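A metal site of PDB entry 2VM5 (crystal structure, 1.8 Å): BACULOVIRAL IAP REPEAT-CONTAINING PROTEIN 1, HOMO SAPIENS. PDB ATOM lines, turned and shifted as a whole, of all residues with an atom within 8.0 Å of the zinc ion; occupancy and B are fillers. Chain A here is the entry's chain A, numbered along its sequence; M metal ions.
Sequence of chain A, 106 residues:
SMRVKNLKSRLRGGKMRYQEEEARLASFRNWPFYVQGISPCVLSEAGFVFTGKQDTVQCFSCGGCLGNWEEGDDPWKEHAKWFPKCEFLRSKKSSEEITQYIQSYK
The zinc ion is bound by NE2 of His 79 (2.2 Å), SG of Cys 62 (2.3 Å), SG of Cys 86 (2.3 Å) and SG of Cys 59 (2.4 Å). The zinc ion has four donor atoms within binding distance.
Within 4 Å of the zinc ion: Cys 59, Cys 62, His 79 and Cys 86. The nearest printed residue that does not touch the zinc ion is Ser 61 (4.6 Å).
SG of Cys 62 sits close to N of Gly 64 (3.5 Å). The backbone carbonyl oxygen (O) of Ala 46 sits at hydrogen-bond distance from a ring nitrogen (ND1) of His 79 (2.7 Å). SG of Cys 59 sits close to N of Ser 61 (3.3 Å). SG of Cys 86 lies close to N of Phe 88 (3.4 Å). The side-chain sulfur (SG) of Cys 86 lies close to the backbone NH (N) of Leu 89 (3.5 Å). The backbone carbonyl oxygen of Gly 64 sits at hydrogen-bond distance from the backbone NH of Cys 59 (2.9 Å).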
ATOM      1  N   ALA A  46       1.033 -26.431  16.509  1.00  0.00           N
ATOM      2  CA  ALA A  46       2.413 -26.027  16.839  1.00  0.00           C
ATOM      3  C   ALA A  46       2.520 -24.748  17.674  1.00  0.00           C
ATOM      4  O   ALA A  46       3.611 -24.240  17.868  1.00  0.00           O
ATOM      5  CB  ALA A  46       3.262 -25.915  15.556  1.00  0.00           C
ATOM      6  N   GLY A  47       1.373 -24.250  18.177  1.00  0.00           N
ATOM      7  CA  GLY A  47       1.327 -23.169  19.160  1.00  0.00           C
ATOM      8  C   GLY A  47       1.056 -21.790  18.561  1.00  0.00           C
ATOM      9  O   GLY A  47       1.010 -20.764  19.279  1.00  0.00           O
ATOM     10  N   PHE A  48       0.882 -21.756  17.247  1.00  0.00           N
ATOM     11  CA  PHE A  48       0.787 -20.482  16.528  1.00  0.00           C
ATOM     12  C   PHE A  48      -0.643 -19.957  16.388  1.00  0.00           C
ATOM     13  O   PHE A  48      -1.590 -20.737  16.184  1.00  0.00           O
ATOM     14  CB  PHE A  48       1.407 -20.556  15.174  1.00  0.00           C
ATOM     15  CG  PHE A  48       2.880 -20.761  15.201  1.00  0.00           C
ATOM     16  CD1 PHE A  48       3.717 -19.741  15.696  1.00  0.00           C
ATOM     17  CD2 PHE A  48       3.426 -21.934  14.744  1.00  0.00           C
ATOM     18  CE1 PHE A  48       5.089 -19.923  15.716  1.00  0.00           C
ATOM     19  CE2 PHE A  48       4.828 -22.137  14.754  1.00  0.00           C
ATOM     20  CZ  PHE A  48       5.652 -21.082  15.247  1.00  0.00           C
ATOM     21  N   GLN A  58       1.953 -15.862  15.438  1.00  0.00           N
ATOM     22  CA  GLN A  58       2.652 -15.654  16.709  1.00  0.00           C
ATOM     23  C   GLN A  58       2.429 -16.817  17.682  1.00  0.00           C
ATOM     24  O   GLN A  58       1.268 -17.246  17.903  1.00  0.00           O
ATOM     25  CB  GLN A  58       2.154 -14.338  17.348  1.00  0.00           C
ATOM     26  CG  GLN A  58       2.874 -13.960  18.680  1.00  0.00           C
ATOM     27  CD  GLN A  58       2.348 -12.640  19.223  1.00  0.00           C
ATOM     28  OE1 GLN A  58       1.926 -11.779  18.462  1.00  0.00           O
ATOM     29  NE2 GLN A  58       2.326 -12.501  20.533  1.00  0.00           N
ATOM     30  N   CYS A  59       3.518 -17.319  18.263  1.00  0.00           N
ATOM     31  CA  CYS A  59       3.379 -18.358  19.293  1.00  0.00           C
ATOM     32  C   CYS A  59       2.648 -17.846  20.546  1.00  0.00           C
ATOM     33  O   CYS A  59       3.027 -16.822  21.065  1.00  0.00           O
ATOM     34  CB  CYS A  59       4.742 -18.891  19.707  1.00  0.00           C
ATOM     35  SG  CYS A  59       4.548 -20.172  20.966  1.00  0.00           S
ATOM     36  N   PHE A  60       1.614 -18.565  21.003  1.00  0.00           N
ATOM     37  CA  PHE A  60       0.857 -18.156  22.194  1.00  0.00           C
ATOM     38  C   PHE A  60       1.726 -18.104  23.472  1.00  0.00           C
ATOM     39  O   PHE A  60       1.384 -17.397  24.435  1.00  0.00           O
ATOM     40  CB  PHE A  60      -0.338 -19.130  22.402  1.00  0.00           C
ATOM     41  CG  PHE A  60       0.031 -20.414  23.120  1.00  0.00           C
ATOM     42  CD1 PHE A  60      -0.125 -20.508  24.531  1.00  0.00           C
ATOM     43  CD2 PHE A  60       0.551 -21.505  22.422  1.00  0.00           C
ATOM     44  CE1 PHE A  60       0.195 -21.688  25.215  1.00  0.00           C
ATOM     45  CE2 PHE A  60       0.884 -22.697  23.107  1.00  0.00           C
ATOM     46  CZ  PHE A  60       0.722 -22.784  24.485  1.00  0.00           C
ATOM     47  N   SER A  61       2.812 -18.865  23.489  1.00  0.00           N
ATOM     48  CA  SER A  61       3.685 -19.026  24.668  1.00  0.00           C
ATOM     49  C   SER A  61       4.897 -18.087  24.606  1.00  0.00           C
ATOM     50  O   SER A  61       5.070 -17.268  25.502  1.00  0.00           O
ATOM     51  CB  SER A  61       4.145 -20.468  24.757  1.00  0.00           C
ATOM     52  OG  SER A  61       5.097 -20.693  25.799  1.00  0.00           O
ATOM     53  N   CYS A  62       5.769 -18.250  23.603  1.00  0.00           N
ATOM     54  CA  CYS A  62       7.027 -17.488  23.485  1.00  0.00           C
ATOM     55  C   CYS A  62       6.934 -16.133  22.749  1.00  0.00           C
ATOM     56  O   CYS A  62       7.870 -15.322  22.775  1.00  0.00           O
ATOM     57  CB  CYS A  62       8.152 -18.354  22.851  1.00  0.00           C
ATOM     58  SG  CYS A  62       7.986 -18.648  21.067  1.00  0.00           S
ATOM     59  N   GLY A  63       5.792 -15.879  22.118  1.00  0.00           N
ATOM     60  CA  GLY A  63       5.615 -14.630  21.365  1.00  0.00           C
ATOM     61  C   GLY A  63       6.413 -14.505  20.070  1.00  0.00           C
ATOM     62  O   GLY A  63       6.344 -13.456  19.426  1.00  0.00           O
ATOM     63  N   GLY A  64       7.131 -15.565  19.676  1.00  0.00           N
ATOM     64  CA  GLY A  64       7.866 -15.600  18.419  1.00  0.00           C
ATOM     65  C   GLY A  64       6.953 -15.417  17.204  1.00  0.00           C
ATOM     66  O   GLY A  64       5.869 -16.002  17.160  1.00  0.00           O
ATOM     67  N   CYS A  65       7.341 -14.599  16.237  1.00  0.00           N
ATOM     68  CA  CYS A  65       6.474 -14.415  15.062  1.00  0.00           C
ATOM     69  C   CYS A  65       7.175 -14.853  13.789  1.00  0.00           C
ATOM     70  O   CYS A  65       8.369 -14.573  13.617  1.00  0.00           O
ATOM     71  CB  CYS A  65       6.030 -12.955  14.921  1.00  0.00           C
ATOM     72  SG  CYS A  65       5.124 -12.257  16.277  1.00  0.00           S
ATOM     73  N   HIS A  79       9.344 -23.474  14.291  1.00  0.00           N
ATOM     74  CA  HIS A  79       9.238 -23.080  15.693  1.00  0.00           C
ATOM     75  C   HIS A  79      10.509 -23.396  16.498  1.00  0.00           C
ATOM     76  O   HIS A  79      11.016 -22.550  17.254  1.00  0.00           O
ATOM     77  CB  HIS A  79       8.018 -23.778  16.324  1.00  0.00           C
ATOM     78  CG  HIS A  79       7.412 -23.043  17.476  1.00  0.00           C
ATOM     79  ND1 HIS A  79       6.077 -23.165  17.800  1.00  0.00           N
ATOM     80  CD2 HIS A  79       7.941 -22.187  18.381  1.00  0.00           C
ATOM     81  CE1 HIS A  79       5.826 -22.448  18.888  1.00  0.00           C
ATOM     82  NE2 HIS A  79       6.926 -21.806  19.231  1.00  0.00           N
ATOM     83  N   ALA A  80      11.004 -24.626  16.336  1.00  0.00           N
ATOM     84  CA  ALA A  80      12.145 -25.142  17.098  1.00  0.00           C
ATOM     85  C   ALA A  80      13.420 -24.430  16.659  1.00  0.00           C
ATOM     86  O   ALA A  80      14.274 -24.142  17.502  1.00  0.00           O
ATOM     87  CB  ALA A  80      12.279 -26.647  16.915  1.00  0.00           C
ATOM     88  N   PHE A  83      12.935 -20.386  17.702  1.00  0.00           N
ATOM     89  CA  PHE A  83      12.563 -19.977  19.069  1.00  0.00           C
ATOM     90  C   PHE A  83      12.889 -21.070  20.068  1.00  0.00           C
ATOM     91  O   PHE A  83      11.989 -21.593  20.752  1.00  0.00           O
ATOM     92  CB  PHE A  83      11.068 -19.633  19.144  1.00  0.00           C
ATOM     93  CG  PHE A  83      10.631 -18.686  18.058  1.00  0.00           C
ATOM     94  CD1 PHE A  83      11.305 -17.456  17.866  1.00  0.00           C
ATOM     95  CD2 PHE A  83       9.585 -19.039  17.202  1.00  0.00           C
ATOM     96  CE1 PHE A  83      10.910 -16.558  16.857  1.00  0.00           C
ATOM     97  CE2 PHE A  83       9.154 -18.153  16.178  1.00  0.00           C
ATOM     98  CZ  PHE A  83       9.866 -16.902  15.997  1.00  0.00           C
ATOM     99  N   PRO A  84      14.178 -21.464  20.130  1.00  0.00           N
ATOM    100  CA  PRO A  84      14.476 -22.694  20.867  1.00  0.00           C
ATOM    101  C   PRO A  84      14.165 -22.673  22.355  1.00  0.00           C
ATOM    102  O   PRO A  84      13.992 -23.752  22.924  1.00  0.00           O
ATOM    103  CB  PRO A  84      15.983 -22.870  20.655  1.00  0.00           C
ATOM    104  CG  PRO A  84      16.484 -21.517  20.383  1.00  0.00           C
ATOM    105  CD  PRO A  84      15.404 -20.917  19.535  1.00  0.00           C
ATOM    106  N   LYS A  85      14.104 -21.494  22.966  1.00  0.00           N
ATOM    107  CA  LYS A  85      13.840 -21.407  24.420  1.00  0.00           C
ATOM    108  C   LYS A  85      12.337 -21.367  24.773  1.00  0.00           C
ATOM    109  O   LYS A  85      11.972 -21.219  25.915  1.00  0.00           O
ATOM    110  CB  LYS A  85      14.518 -20.190  25.072  1.00  0.00           C
ATOM    111  CG  LYS A  85      16.013 -20.073  24.768  1.00  0.00           C
ATOM    112  CD  LYS A  85      16.650 -19.205  25.832  1.00  0.00           C
ATOM    113  CE  LYS A  85      16.694 -17.776  25.379  1.00  0.00           C
ATOM    114  NZ  LYS A  85      17.739 -17.135  26.230  1.00  0.00           N
ATOM    115  N   CYS A  86      11.467 -21.516  23.767  1.00  0.00           N
ATOM    116  CA  CYS A  86      10.030 -21.536  23.987  1.00  0.00           C
ATOM    117  C   CYS A  86       9.595 -22.594  25.020  1.00  0.00           C
ATOM    118  O   CYS A  86       9.921 -23.783  24.890  1.00  0.00           O
ATOM    119  CB  CYS A  86       9.316 -21.869  22.659  1.00  0.00           C
ATOM    120  SG  CYS A  86       7.569 -21.995  22.858  1.00  0.00           S
ATOM    121  N   GLU A  87       8.875 -22.163  26.054  1.00  0.00           N
ATOM    122  CA  GLU A  87       8.445 -23.085  27.118  1.00  0.00           C
ATOM    123  C   GLU A  87       7.440 -24.123  26.600  1.00  0.00           C
ATOM    124  O   GLU A  87       7.396 -25.279  27.069  1.00  0.00           O
ATOM    125  CB  GLU A  87       7.799 -22.340  28.280  1.00  0.00           C
ATOM    126  CG  GLU A  87       7.625 -23.252  29.502  1.00  0.00           C
ATOM    127  CD  GLU A  87       6.815 -22.654  30.674  1.00  0.00           C
ATOM    128  OE1 GLU A  87       6.261 -23.462  31.462  1.00  0.00           O
ATOM    129  OE2 GLU A  87       6.737 -21.409  30.841  1.00  0.00           O
ATOM    130  N   PHE A  88       6.572 -23.687  25.683  1.00  0.00           N
ATOM    131  CA  PHE A  88       5.633 -24.642  25.028  1.00  0.00           C
ATOM    132  C   PHE A  88       6.409 -25.785  24.329  1.00  0.00           C
ATOM    133  O   PHE A  88       6.094 -26.968  24.501  1.00  0.00           O
ATOM    134  CB  PHE A  88       4.703 -23.885  24.065  1.00  0.00           C
ATOM    135  CG  PHE A  88       3.937 -24.778  23.119  1.00  0.00           C
ATOM    136  CD1 PHE A  88       2.802 -25.483  23.572  1.00  0.00           C
ATOM    137  CD2 PHE A  88       4.326 -24.888  21.778  1.00  0.00           C
ATOM    138  CE1 PHE A  88       2.070 -26.292  22.677  1.00  0.00           C
ATOM    139  CE2 PHE A  88       3.615 -25.678  20.883  1.00  0.00           C
ATOM    140  CZ  PHE A  88       2.498 -26.403  21.346  1.00  0.00           C
ATOM    141  N   LEU A  89       7.429 -25.451  23.537  1.00  0.00           N
ATOM    142  CA  LEU A  89       8.249 -26.499  22.889  1.00  0.00           C
ATOM    143  C   LEU A  89       8.937 -27.396  23.902  1.00  0.00           C
ATOM    144  O   LEU A  89       8.967 -28.613  23.756  1.00  0.00           O
ATOM    145  CB  LEU A  89       9.309 -25.882  21.977  1.00  0.00           C
ATOM    146  CG  LEU A  89       8.773 -25.189  20.716  1.00  0.00           C
ATOM    147  CD1 LEU A  89       9.922 -24.867  19.750  1.00  0.00           C
ATOM    148  CD2 LEU A  89       7.656 -26.048  19.994  1.00  0.00           C
ATOM    149  N   ARG A  90       9.509 -26.776  24.937  1.00  0.00           N
ATOM    150  CA  ARG A  90      10.142 -27.587  25.974  1.00  0.00           C
ATOM    151  C   ARG A  90       9.140 -28.536  26.665  1.00  0.00           C
ATOM    152  O   ARG A  90       9.496 -29.690  26.983  1.00  0.00           O
ATOM    153  CB  ARG A  90      10.860 -26.688  26.965  1.00  0.00           C
ATOM    154  CG  ARG A  90      11.747 -27.475  27.971  1.00  0.00           C
ATOM    155  CD  ARG A  90      12.736 -26.536  28.727  1.00  0.00           C
ATOM    156  NE  ARG A  90      12.089 -25.424  29.404  1.00  0.00           N
ATOM    157  CZ  ARG A  90      12.022 -24.174  28.933  1.00  0.00           C
ATOM    158  NH1 ARG A  90      11.415 -23.229  29.648  1.00  0.00           N
ATOM    159  NH2 ARG A  90      12.533 -23.849  27.757  1.00  0.00           N
HETATM  160 ZN    ZN M   1       6.889 -20.661  21.057  1.00  0.00          ZN
